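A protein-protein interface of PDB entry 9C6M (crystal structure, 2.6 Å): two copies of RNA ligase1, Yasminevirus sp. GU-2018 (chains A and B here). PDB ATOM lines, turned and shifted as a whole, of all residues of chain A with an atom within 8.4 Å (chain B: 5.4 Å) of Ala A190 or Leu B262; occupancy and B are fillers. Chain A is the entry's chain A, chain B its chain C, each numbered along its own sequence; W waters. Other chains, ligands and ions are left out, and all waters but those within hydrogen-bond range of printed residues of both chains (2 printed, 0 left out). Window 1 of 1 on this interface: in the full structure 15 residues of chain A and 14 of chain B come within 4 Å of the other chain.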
ATOM      1  N   TRP A 127     -25.203  -8.376  15.486  1.00  0.00           N
ATOM      2  CA  TRP A 127     -24.059  -8.386  14.584  1.00  0.00           C
ATOM      3  C   TRP A 127     -24.020  -9.602  13.671  1.00  0.00           C
ATOM      4  O   TRP A 127     -23.342  -9.555  12.640  1.00  0.00           O
ATOM      5  CB  TRP A 127     -22.764  -8.288  15.394  1.00  0.00           C
ATOM      6  CG  TRP A 127     -22.797  -7.105  16.303  1.00  0.00           C
ATOM      7  CD1 TRP A 127     -22.696  -7.109  17.660  1.00  0.00           C
ATOM      8  CD2 TRP A 127     -22.984  -5.738  15.917  1.00  0.00           C
ATOM      9  NE1 TRP A 127     -22.794  -5.826  18.147  1.00  0.00           N
ATOM     10  CE2 TRP A 127     -22.974  -4.967  17.096  1.00  0.00           C
ATOM     11  CE3 TRP A 127     -23.157  -5.091  14.689  1.00  0.00           C
ATOM     12  CZ2 TRP A 127     -23.125  -3.581  17.082  1.00  0.00           C
ATOM     13  CZ3 TRP A 127     -23.307  -3.718  14.677  1.00  0.00           C
ATOM     14  CH2 TRP A 127     -23.291  -2.976  15.867  1.00  0.00           C
ATOM     15  N   ASP A 130     -26.127  -8.232  11.094  1.00  0.00           N
ATOM     16  CA  ASP A 130     -25.509  -7.059  10.491  1.00  0.00           C
ATOM     17  C   ASP A 130     -24.671  -7.385   9.265  1.00  0.00           C
ATOM     18  O   ASP A 130     -24.209  -6.456   8.592  1.00  0.00           O
ATOM     19  CB  ASP A 130     -24.639  -6.332  11.517  1.00  0.00           C
ATOM     20  CG  ASP A 130     -24.113  -5.012  10.999  1.00  0.00           C
ATOM     21  OD1 ASP A 130     -24.908  -4.232  10.436  1.00  0.00           O
ATOM     22  OD2 ASP A 130     -22.906  -4.748  11.162  1.00  0.00           O
ATOM     23  N   CYS A 131     -24.455  -8.655   8.947  1.00  0.00           N
ATOM     24  CA  CYS A 131     -23.773  -8.987   7.704  1.00  0.00           C
ATOM     25  C   CYS A 131     -24.732  -9.037   6.518  1.00  0.00           C
ATOM     26  O   CYS A 131     -24.280  -9.197   5.380  1.00  0.00           O
ATOM     27  CB  CYS A 131     -23.012 -10.310   7.844  1.00  0.00           C
ATOM     28  SG  CYS A 131     -24.006 -11.806   7.734  1.00  0.00           S
ATOM     29  N   LYS A 134     -28.001  -3.825   3.953  1.00  0.00           N
ATOM     30  CA  LYS A 134     -29.049  -2.935   4.434  1.00  0.00           C
ATOM     31  C   LYS A 134     -29.990  -2.565   3.291  1.00  0.00           C
ATOM     32  O   LYS A 134     -29.581  -2.451   2.131  1.00  0.00           O
ATOM     33  CB  LYS A 134     -28.433  -1.688   5.063  1.00  0.00           C
ATOM     34  CG  LYS A 134     -27.409  -1.997   6.161  1.00  0.00           C
ATOM     35  CD  LYS A 134     -28.009  -2.856   7.277  1.00  0.00           C
ATOM     36  CE  LYS A 134     -26.959  -3.288   8.295  1.00  0.00           C
ATOM     37  NZ  LYS A 134     -25.937  -4.202   7.706  1.00  0.00           N
ATOM     38  N   LEU A 148     -23.186  -9.738   2.867  1.00  0.00           N
ATOM     39  CA  LEU A 148     -21.821  -9.395   2.502  1.00  0.00           C
ATOM     40  C   LEU A 148     -20.910 -10.571   2.826  1.00  0.00           C
ATOM     41  O   LEU A 148     -20.975 -11.130   3.926  1.00  0.00           O
ATOM     42  CB  LEU A 148     -21.350  -8.150   3.249  1.00  0.00           C
ATOM     43  CG  LEU A 148     -19.945  -7.668   2.878  1.00  0.00           C
ATOM     44  CD1 LEU A 148     -19.913  -7.164   1.438  1.00  0.00           C
ATOM     45  CD2 LEU A 148     -19.466  -6.589   3.837  1.00  0.00           C
ATOM     46  N   CYS A 149     -20.065 -10.947   1.873  1.00  0.00           N
ATOM     47  CA  CYS A 149     -19.108 -12.020   2.084  1.00  0.00           C
ATOM     48  C   CYS A 149     -17.766 -11.617   1.496  1.00  0.00           C
ATOM     49  O   CYS A 149     -17.693 -10.795   0.578  1.00  0.00           O
ATOM     50  CB  CYS A 149     -19.565 -13.331   1.441  1.00  0.00           C
ATOM     51  SG  CYS A 149     -19.155 -13.423  -0.304  1.00  0.00           S
ATOM     52  N   ILE A 150     -16.703 -12.203   2.032  1.00  0.00           N
ATOM     53  CA  ILE A 150     -15.355 -12.018   1.512  1.00  0.00           C
ATOM     54  C   ILE A 150     -14.964 -13.314   0.817  1.00  0.00           C
ATOM     55  O   ILE A 150     -15.022 -14.395   1.416  1.00  0.00           O
ATOM     56  CB  ILE A 150     -14.362 -11.632   2.618  1.00  0.00           C
ATOM     57  CG1 ILE A 150     -12.976 -11.374   2.025  1.00  0.00           C
ATOM     58  CG2 ILE A 150     -14.287 -12.706   3.686  1.00  0.00           C
ATOM     59  CD1 ILE A 150     -12.066 -10.572   2.935  1.00  0.00           C
ATOM     60  N   TYR A 161     -14.357  -8.107  -1.057  1.00  0.00           N
ATOM     61  CA  TYR A 161     -15.685  -8.094  -0.464  1.00  0.00           C
ATOM     62  C   TYR A 161     -16.720  -8.057  -1.584  1.00  0.00           C
ATOM     63  O   TYR A 161     -16.518  -7.402  -2.612  1.00  0.00           O
ATOM     64  CB  TYR A 161     -15.873  -6.885   0.454  1.00  0.00           C
ATOM     65  CG  TYR A 161     -14.844  -6.708   1.558  1.00  0.00           C
ATOM     66  CD1 TYR A 161     -13.632  -6.073   1.311  1.00  0.00           C
ATOM     67  CD2 TYR A 161     -15.104  -7.132   2.856  1.00  0.00           C
ATOM     68  CE1 TYR A 161     -12.701  -5.888   2.318  1.00  0.00           C
ATOM     69  CE2 TYR A 161     -14.178  -6.948   3.870  1.00  0.00           C
ATOM     70  CZ  TYR A 161     -12.979  -6.325   3.594  1.00  0.00           C
ATOM     71  OH  TYR A 161     -12.051  -6.138   4.594  1.00  0.00           O
ATOM     72  N   GLU A 163     -21.213  -8.426  -2.292  1.00  0.00           N
ATOM     73  CA  GLU A 163     -22.594  -8.658  -1.884  1.00  0.00           C
ATOM     74  C   GLU A 163     -23.166  -9.795  -2.722  1.00  0.00           C
ATOM     75  O   GLU A 163     -23.241  -9.688  -3.951  1.00  0.00           O
ATOM     76  CB  GLU A 163     -23.428  -7.389  -2.056  1.00  0.00           C
ATOM     77  CG  GLU A 163     -23.011  -6.232  -1.157  1.00  0.00           C
ATOM     78  CD  GLU A 163     -23.913  -5.013  -1.296  1.00  0.00           C
ATOM     79  OE1 GLU A 163     -24.883  -5.068  -2.084  1.00  0.00           O
ATOM     80  OE2 GLU A 163     -23.649  -3.998  -0.616  1.00  0.00           O
ATOM     81  N   LEU A 176     -18.247 -16.193  10.278  1.00  0.00           N
ATOM     82  CA  LEU A 176     -18.720 -14.820  10.379  1.00  0.00           C
ATOM     83  C   LEU A 176     -17.673 -13.992  11.111  1.00  0.00           C
ATOM     84  O   LEU A 176     -17.251 -14.351  12.215  1.00  0.00           O
ATOM     85  CB  LEU A 176     -20.062 -14.772  11.110  1.00  0.00           C
ATOM     86  CG  LEU A 176     -20.558 -13.419  11.620  1.00  0.00           C
ATOM     87  CD1 LEU A 176     -20.703 -12.418  10.490  1.00  0.00           C
ATOM     88  CD2 LEU A 176     -21.884 -13.596  12.354  1.00  0.00           C
ATOM     89  N   MET A 177     -17.253 -12.892  10.492  1.00  0.00           N
ATOM     90  CA  MET A 177     -16.144 -12.106  11.016  1.00  0.00           C
ATOM     91  C   MET A 177     -16.430 -10.613  10.993  1.00  0.00           C
ATOM     92  O   MET A 177     -17.449 -10.182  10.457  1.00  0.00           O
ATOM     93  CB  MET A 177     -14.877 -12.382  10.205  1.00  0.00           C
ATOM     94  CG  MET A 177     -14.539 -13.849  10.053  1.00  0.00           C
ATOM     95  SD  MET A 177     -13.147 -14.105   8.717  1.00  0.00           S
ATOM     96  CE  MET A 177     -14.147 -13.664   7.099  1.00  0.00           C
ATOM     97  N   GLY A 178     -15.522  -9.831  11.580  1.00  0.00           N
ATOM     98  CA  GLY A 178     -15.615  -8.393  11.536  1.00  0.00           C
ATOM     99  C   GLY A 178     -15.420  -7.718  12.879  1.00  0.00           C
ATOM    100  O   GLY A 178     -15.003  -8.331  13.868  1.00  0.00           O
ATOM    101  N   PRO A 179     -15.733  -6.418  12.932  1.00  0.00           N
ATOM    102  CA  PRO A 179     -15.479  -5.630  14.143  1.00  0.00           C
ATOM    103  C   PRO A 179     -15.881  -6.275  15.466  1.00  0.00           C
ATOM    104  O   PRO A 179     -15.095  -6.252  16.418  1.00  0.00           O
ATOM    105  CB  PRO A 179     -16.295  -4.354  13.882  1.00  0.00           C
ATOM    106  CG  PRO A 179     -16.183  -4.175  12.391  1.00  0.00           C
ATOM    107  CD  PRO A 179     -16.158  -5.569  11.798  1.00  0.00           C
ATOM    108  N   LYS A 180     -17.082  -6.846  15.550  1.00  0.00           N
ATOM    109  CA  LYS A 180     -17.637  -7.286  16.823  1.00  0.00           C
ATOM    110  C   LYS A 180     -17.448  -8.779  17.070  1.00  0.00           C
ATOM    111  O   LYS A 180     -18.166  -9.360  17.891  1.00  0.00           O
ATOM    112  CB  LYS A 180     -19.122  -6.926  16.894  1.00  0.00           C
ATOM    113  CG  LYS A 180     -19.395  -5.438  17.066  1.00  0.00           C
ATOM    114  CD  LYS A 180     -19.427  -5.054  18.540  1.00  0.00           C
ATOM    115  CE  LYS A 180     -19.723  -3.575  18.732  1.00  0.00           C
ATOM    116  NZ  LYS A 180     -18.578  -2.725  18.306  1.00  0.00           N
ATOM    117  N   PHE A 181     -16.491  -9.408  16.394  1.00  0.00           N
ATOM    118  CA  PHE A 181     -16.217 -10.831  16.576  1.00  0.00           C
ATOM    119  C   PHE A 181     -14.724 -11.024  16.795  1.00  0.00           C
ATOM    120  O   PHE A 181     -13.917 -10.768  15.895  1.00  0.00           O
ATOM    121  CB  PHE A 181     -16.719 -11.639  15.379  1.00  0.00           C
ATOM    122  CG  PHE A 181     -18.213 -11.603  15.220  1.00  0.00           C
ATOM    123  CD1 PHE A 181     -19.020 -12.434  15.973  1.00  0.00           C
ATOM    124  CD2 PHE A 181     -18.809 -10.728  14.332  1.00  0.00           C
ATOM    125  CE1 PHE A 181     -20.390 -12.399  15.839  1.00  0.00           C
ATOM    126  CE2 PHE A 181     -20.182 -10.691  14.193  1.00  0.00           C
ATOM    127  CZ  PHE A 181     -20.972 -11.528  14.949  1.00  0.00           C
ATOM    128  N   ASN A 184     -11.893  -8.339  15.864  1.00  0.00           N
ATOM    129  CA  ASN A 184     -11.497  -8.058  14.490  1.00  0.00           C
ATOM    130  C   ASN A 184      -9.986  -8.216  14.299  1.00  0.00           C
ATOM    131  O   ASN A 184      -9.305  -7.274  13.882  1.00  0.00           O
ATOM    132  CB  ASN A 184     -11.953  -6.661  14.087  1.00  0.00           C
ATOM    133  CG  ASN A 184     -11.982  -6.458  12.580  1.00  0.00           C
ATOM    134  OD1 ASN A 184     -11.829  -7.403  11.806  1.00  0.00           O
ATOM    135  ND2 ASN A 184     -12.193  -5.216  12.160  1.00  0.00           N
ATOM    136  N   GLY A 187      -8.739  -7.244  10.788  1.00  0.00           N
ATOM    137  CA  GLY A 187      -8.843  -5.887  10.284  1.00  0.00           C
ATOM    138  C   GLY A 187      -9.872  -5.715   9.192  1.00  0.00           C
ATOM    139  O   GLY A 187      -9.697  -4.869   8.307  1.00  0.00           O
ATOM    140  N   LEU A 188     -10.944  -6.497   9.226  1.00  0.00           N
ATOM    141  CA  LEU A 188     -11.985  -6.371   8.219  1.00  0.00           C
ATOM    142  C   LEU A 188     -12.745  -5.062   8.399  1.00  0.00           C
ATOM    143  O   LEU A 188     -12.930  -4.568   9.515  1.00  0.00           O
ATOM    144  CB  LEU A 188     -12.944  -7.556   8.299  1.00  0.00           C
ATOM    145  CG  LEU A 188     -12.277  -8.918   8.103  1.00  0.00           C
ATOM    146  CD1 LEU A 188     -13.252 -10.044   8.395  1.00  0.00           C
ATOM    147  CD2 LEU A 188     -11.720  -9.041   6.691  1.00  0.00           C
ATOM    148  N   LYS A 189     -13.187  -4.499   7.281  1.00  0.00           N
ATOM    149  CA  LYS A 189     -13.885  -3.223   7.273  1.00  0.00           C
ATOM    150  C   LYS A 189     -15.384  -3.352   7.522  1.00  0.00           C
ATOM    151  O   LYS A 189     -16.079  -2.332   7.540  1.00  0.00           O
ATOM    152  CB  LYS A 189     -13.650  -2.513   5.935  1.00  0.00           C
ATOM    153  CG  LYS A 189     -12.226  -2.027   5.740  1.00  0.00           C
ATOM    154  CD  LYS A 189     -12.005  -1.461   4.346  1.00  0.00           C
ATOM    155  CE  LYS A 189     -11.505  -2.527   3.380  1.00  0.00           C
ATOM    156  NZ  LYS A 189     -10.207  -3.127   3.812  1.00  0.00           N
ATOM    157  N   ALA A 190     -15.898  -4.562   7.718  1.00  0.00           N
ATOM    158  CA  ALA A 190     -17.332  -4.747   7.906  1.00  0.00           C
ATOM    159  C   ALA A 190     -17.600  -6.205   8.246  1.00  0.00           C
ATOM    160  O   ALA A 190     -16.775  -7.083   7.980  1.00  0.00           O
ATOM    161  CB  ALA A 190     -18.117  -4.336   6.656  1.00  0.00           C
ATOM    162  N   HIS A 191     -18.770  -6.447   8.837  1.00  0.00           N
ATOM    163  CA  HIS A 191     -19.183  -7.804   9.178  1.00  0.00           C
ATOM    164  C   HIS A 191     -19.527  -8.570   7.908  1.00  0.00           C
ATOM    165  O   HIS A 191     -20.383  -8.138   7.129  1.00  0.00           O
ATOM    166  CB  HIS A 191     -20.379  -7.772  10.121  1.00  0.00           C
ATOM    167  CG  HIS A 191     -20.066  -7.201  11.467  1.00  0.00           C
ATOM    168  ND1 HIS A 191     -20.818  -6.200  12.044  1.00  0.00           N
ATOM    169  CD2 HIS A 191     -19.081  -7.488  12.349  1.00  0.00           C
ATOM    170  CE1 HIS A 191     -20.307  -5.894  13.223  1.00  0.00           C
ATOM    171  NE2 HIS A 191     -19.252  -6.660  13.431  1.00  0.00           N
ATOM    172  N   CYS A 192     -18.874  -9.713   7.709  1.00  0.00           N
ATOM    173  CA  CYS A 192     -19.019 -10.470   6.476  1.00  0.00           C
ATOM    174  C   CYS A 192     -18.930 -11.959   6.775  1.00  0.00           C
ATOM    175  O   CYS A 192     -18.576 -12.376   7.880  1.00  0.00           O
ATOM    176  CB  CYS A 192     -17.951 -10.064   5.458  1.00  0.00           C
ATOM    177  SG  CYS A 192     -16.282 -10.103   6.135  1.00  0.00           S
ATOM    178  N   LEU A 193     -19.263 -12.759   5.765  1.00  0.00           N
ATOM    179  CA  LEU A 193     -19.180 -14.208   5.830  1.00  0.00           C
ATOM    180  C   LEU A 193     -18.092 -14.704   4.886  1.00  0.00           C
ATOM    181  O   LEU A 193     -17.818 -14.090   3.852  1.00  0.00           O
ATOM    182  CB  LEU A 193     -20.515 -14.856   5.449  1.00  0.00           C
ATOM    183  CG  LEU A 193     -21.739 -14.458   6.270  1.00  0.00           C
ATOM    184  CD1 LEU A 193     -22.983 -15.084   5.671  1.00  0.00           C
ATOM    185  CD2 LEU A 193     -21.582 -14.875   7.719  1.00  0.00           C
ATOM    186  N   ASP A 273      -7.722  -8.886   4.284  1.00  0.00           N
ATOM    187  CA  ASP A 273      -8.127  -8.460   2.948  1.00  0.00           C
ATOM    188  C   ASP A 273      -6.939  -8.230   2.023  1.00  0.00           C
ATOM    189  O   ASP A 273      -7.136  -8.140   0.807  1.00  0.00           O
ATOM    190  CB  ASP A 273      -9.003  -7.197   2.991  1.00  0.00           C
ATOM    191  CG  ASP A 273      -8.468  -6.121   3.911  1.00  0.00           C
ATOM    192  OD1 ASP A 273      -7.303  -5.702   3.748  1.00  0.00           O
ATOM    193  OD2 ASP A 273      -9.244  -5.666   4.781  1.00  0.00           O
ATOM    194  N   ARG B 228     -19.807   2.069  -1.857  1.00  0.00           N
ATOM    195  CA  ARG B 228     -19.422   1.117  -0.822  1.00  0.00           C
ATOM    196  C   ARG B 228     -18.395   0.130  -1.354  1.00  0.00           C
ATOM    197  O   ARG B 228     -17.472  -0.268  -0.633  1.00  0.00           O
ATOM    198  CB  ARG B 228     -20.661   0.385  -0.306  1.00  0.00           C
ATOM    199  CG  ARG B 228     -20.409  -0.538   0.880  1.00  0.00           C
ATOM    200  CD  ARG B 228     -21.720  -1.120   1.392  1.00  0.00           C
ATOM    201  NE  ARG B 228     -21.620  -1.630   2.756  1.00  0.00           N
ATOM    202  CZ  ARG B 228     -21.773  -2.900   3.108  1.00  0.00           C
ATOM    203  NH1 ARG B 228     -22.023  -3.845   2.214  1.00  0.00           N
ATOM    204  NH2 ARG B 228     -21.685  -3.231   4.394  1.00  0.00           N
ATOM    205  N   PHE B 231     -14.772   1.657  -1.444  1.00  0.00           N
ATOM    206  CA  PHE B 231     -14.078   1.678  -0.160  1.00  0.00           C
ATOM    207  C   PHE B 231     -13.618   0.282   0.241  1.00  0.00           C
ATOM    208  O   PHE B 231     -12.537   0.121   0.817  1.00  0.00           O
ATOM    209  CB  PHE B 231     -14.983   2.281   0.915  1.00  0.00           C
ATOM    210  CG  PHE B 231     -15.008   3.783   0.906  1.00  0.00           C
ATOM    211  CD1 PHE B 231     -15.913   4.473   0.118  1.00  0.00           C
ATOM    212  CD2 PHE B 231     -14.115   4.506   1.678  1.00  0.00           C
ATOM    213  CE1 PHE B 231     -15.931   5.858   0.105  1.00  0.00           C
ATOM    214  CE2 PHE B 231     -14.126   5.887   1.669  1.00  0.00           C
ATOM    215  CZ  PHE B 231     -15.036   6.564   0.881  1.00  0.00           C
ATOM    216  N   LEU B 232     -14.412  -0.741  -0.072  1.00  0.00           N
ATOM    217  CA  LEU B 232     -14.056  -2.093   0.339  1.00  0.00           C
ATOM    218  C   LEU B 232     -12.894  -2.643  -0.481  1.00  0.00           C
ATOM    219  O   LEU B 232     -12.004  -3.305   0.066  1.00  0.00           O
ATOM    220  CB  LEU B 232     -15.271  -3.012   0.222  1.00  0.00           C
ATOM    221  CG  LEU B 232     -16.366  -2.826   1.275  1.00  0.00           C
ATOM    222  CD1 LEU B 232     -17.594  -3.642   0.916  1.00  0.00           C
ATOM    223  CD2 LEU B 232     -15.861  -3.211   2.657  1.00  0.00           C
ATOM    224  N   ARG B 257     -17.615   6.467   6.328  1.00  0.00           N
ATOM    225  CA  ARG B 257     -17.761   5.020   6.247  1.00  0.00           C
ATOM    226  C   ARG B 257     -19.030   4.532   6.935  1.00  0.00           C
ATOM    227  O   ARG B 257     -19.533   3.455   6.595  1.00  0.00           O
ATOM    228  CB  ARG B 257     -16.550   4.325   6.867  1.00  0.00           C
ATOM    229  CG  ARG B 257     -15.389   4.091   5.910  1.00  0.00           C
ATOM    230  CD  ARG B 257     -14.486   2.995   6.458  1.00  0.00           C
ATOM    231  NE  ARG B 257     -13.190   2.916   5.798  1.00  0.00           N
ATOM    232  CZ  ARG B 257     -12.210   2.110   6.187  1.00  0.00           C
ATOM    233  NH1 ARG B 257     -12.354   1.301   7.225  1.00  0.00           N
ATOM    234  NH2 ARG B 257     -11.059   2.116   5.523  1.00  0.00           N
ATOM    235  N   HIS B 258     -19.556   5.296   7.896  1.00  0.00           N
ATOM    236  CA  HIS B 258     -20.752   4.864   8.610  1.00  0.00           C
ATOM    237  C   HIS B 258     -21.991   4.963   7.730  1.00  0.00           C
ATOM    238  O   HIS B 258     -22.924   4.166   7.888  1.00  0.00           O
ATOM    239  CB  HIS B 258     -20.918   5.688   9.886  1.00  0.00           C
ATOM    240  CG  HIS B 258     -19.836   5.456  10.898  1.00  0.00           C
ATOM    241  ND1 HIS B 258     -19.548   6.354  11.902  1.00  0.00           N
ATOM    242  CD2 HIS B 258     -18.975   4.423  11.060  1.00  0.00           C
ATOM    243  CE1 HIS B 258     -18.556   5.887  12.637  1.00  0.00           C
ATOM    244  NE2 HIS B 258     -18.190   4.716  12.148  1.00  0.00           N
ATOM    245  N   LEU B 260     -21.957   4.171   4.675  1.00  0.00           N
ATOM    246  CA  LEU B 260     -21.831   2.996   3.829  1.00  0.00           C
ATOM    247  C   LEU B 260     -21.902   1.694   4.616  1.00  0.00           C
ATOM    248  O   LEU B 260     -21.527   0.643   4.085  1.00  0.00           O
ATOM    249  CB  LEU B 260     -20.514   3.051   3.052  1.00  0.00           C
ATOM    250  CG  LEU B 260     -20.239   4.371   2.333  1.00  0.00           C
ATOM    251  CD1 LEU B 260     -18.934   4.298   1.566  1.00  0.00           C
ATOM    252  CD2 LEU B 260     -21.385   4.722   1.405  1.00  0.00           C
ATOM    253  N   ASP B 261     -22.361   1.737   5.865  1.00  0.00           N
ATOM    254  CA  ASP B 261     -22.456   0.532   6.684  1.00  0.00           C
ATOM    255  C   ASP B 261     -21.090  -0.141   6.805  1.00  0.00           C
ATOM    256  O   ASP B 261     -20.970  -1.366   6.743  1.00  0.00           O
ATOM    257  CB  ASP B 261     -23.502  -0.428   6.108  1.00  0.00           C
ATOM    258  CG  ASP B 261     -23.895  -1.526   7.081  1.00  0.00           C
ATOM    259  OD1 ASP B 261     -24.093  -1.223   8.277  1.00  0.00           O
ATOM    260  OD2 ASP B 261     -24.025  -2.690   6.644  1.00  0.00           O
ATOM    261  N   LEU B 262     -20.047   0.675   6.966  1.00  0.00           N
ATOM    262  CA  LEU B 262     -18.685   0.198   7.136  1.00  0.00           C
ATOM    263  C   LEU B 262     -18.117   0.689   8.463  1.00  0.00           C
ATOM    264  O   LEU B 262     -18.629   1.629   9.078  1.00  0.00           O
ATOM    265  CB  LEU B 262     -17.773   0.665   5.992  1.00  0.00           C
ATOM    266  CG  LEU B 262     -18.101   0.175   4.582  1.00  0.00           C
ATOM    267  CD1 LEU B 262     -17.155   0.796   3.564  1.00  0.00           C
ATOM    268  CD2 LEU B 262     -18.031  -1.337   4.511  1.00  0.00           C
ATOM    269  N   GLU B 263     -17.035   0.038   8.885  1.00  0.00           N
ATOM    270  CA  GLU B 263     -16.353   0.351  10.131  1.00  0.00           C
ATOM    271  C   GLU B 263     -15.211   1.325   9.871  1.00  0.00           C
ATOM    272  O   GLU B 263     -14.532   1.242   8.844  1.00  0.00           O
ATOM    273  CB  GLU B 263     -15.812  -0.933  10.765  1.00  0.00           C
ATOM    274  CG  GLU B 263     -15.067  -0.757  12.080  1.00  0.00           C
ATOM    275  CD  GLU B 263     -15.977  -0.877  13.281  1.00  0.00           C
ATOM    276  OE1 GLU B 263     -17.211  -0.867  13.092  1.00  0.00           O
ATOM    277  OE2 GLU B 263     -15.461  -0.988  14.413  1.00  0.00           O
ATOM    278  N   TRP B 264     -15.003   2.250  10.804  1.00  0.00           N
ATOM    279  CA  TRP B 264     -13.827   3.112  10.796  1.00  0.00           C
ATOM    280  C   TRP B 264     -13.108   2.972  12.130  1.00  0.00           C
ATOM    281  O   TRP B 264     -13.673   3.296  13.181  1.00  0.00           O
ATOM    282  CB  TRP B 264     -14.184   4.577  10.540  1.00  0.00           C
ATOM    283  CG  TRP B 264     -12.961   5.455  10.558  1.00  0.00           C
ATOM    284  CD1 TRP B 264     -12.706   6.491  11.408  1.00  0.00           C
ATOM    285  CD2 TRP B 264     -11.817   5.349   9.701  1.00  0.00           C
ATOM    286  NE1 TRP B 264     -11.479   7.044  11.126  1.00  0.00           N
ATOM    287  CE2 TRP B 264     -10.913   6.360  10.082  1.00  0.00           C
ATOM    288  CE3 TRP B 264     -11.472   4.501   8.644  1.00  0.00           C
ATOM    289  CZ2 TRP B 264      -9.686   6.546   9.446  1.00  0.00           C
ATOM    290  CZ3 TRP B 264     -10.256   4.688   8.011  1.00  0.00           C
ATOM    291  CH2 TRP B 264      -9.378   5.702   8.415  1.00  0.00           C
HETATM  292  O   HOH W   1     -23.053  -2.204  10.394  1.00  0.00           O
HETATM  293  O   HOH W   2     -12.660  -2.789  14.330  1.00  0.00           O
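NZ of Lys A134 is in salt-bridge range of OD2 of Asp B261, at 2.7 Å.
O of Lys A189 lies within hydrogen-bond range of N of Glu B263 (2.9 Å).
The guanidinium group (NH1) of Arg B228 lies within salt-bridge range of the side-chain carboxylate (OE2) of Glu A163 (3.3 Å).
The guanidinium group of Arg B257 sits at hydrogen-bond distance from the backbone carbonyl oxygen of Glu B263 (2.7 Å).
The side-chain sulfur (SG) of Cys A192 sits at hydrogen-bond distance from the backbone carbonyl oxygen (O) of Ala A190 (3.6 Å).
The side-chain hydroxyl of Tyr A161 lies within hydrogen-bond range of the side-chain carboxylate of Asp A273 (2.9 Å).
NZ of Lys A189 lies within salt-bridge range of OD2 of Asp A273 (2.9 Å).
The side-chain hydroxyl (OH) of Tyr A161 sits at hydrogen-bond distance from the backbone NH (N) of Lys A189 (3.3 Å).
The side-chain carboxylate of Asp B261 lies within salt-bridge range of the guanidinium group of Arg B228 (3.3 Å).
Among the printed residues, pairs that only touch across the chains: Pro A179 with Glu B263 (3.4 Å), Lys A189 with Leu B232 (3.4 Å), Tyr A161 with Leu B232 (3.4 Å), Lys A189 with Arg B257 (3.6 Å), Lys A189 with Leu B262 (3.7 Å), Ala A190 with Leu B262 (3.7 Å), Asp A130 with Asp B261 (3.8 Å) and Lys A189 with Phe B231 (3.8 Å).
Ala A190 touches just one residue of chain B: Leu B262.
Of the printed residues of chain A, Glu B263 touches Pro A179 and Lys A189.
Printed residues of chain A within 4 Å of Leu B232: Tyr A161 and Lys A189.
Of the printed residues of chain A, Arg B228 touches Glu A163 (3.3 Å).
Of the printed residues of chain B, Pro A179 touches Glu B263.
Cys A131 touches none of the printed residues of chain B.
Gly A187 touches none of the printed residues of chain B.
The nearest residue of chain B that does not touch Ala A190 is Asp B261 (4.1 Å).
Printed residues of chain B that touch a printed residue of chain A: Arg B228, Phe B231, Leu B232, Arg B257, Asp B261, Leu B262 and Glu B263.
Among the printed residues, 11 pairs touch across the chains.
Among the printed residues, Asp or Glu carboxylates within 4 Å of a Lys or Arg side-chain nitrogen of the other chain: Lys A134 with Asp B261 (2.7 Å) and Glu A163 with Arg B228 (3.3 Å).
No position is printed for both chains.
Of the 11 pairs that touch across the chains among the printed residues, none has its exchanged pair printed and touching as well.
Water W1 lies within hydrogen-bond range of OD1 of Asp B261 (2.6 Å) and OD2 of Asp A130 (2.7 Å).
Water W2 lies within hydrogen-bond range of ND2 of Asn A184 (3.3 Å) and OE2 of Glu B263 (3.3 Å).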
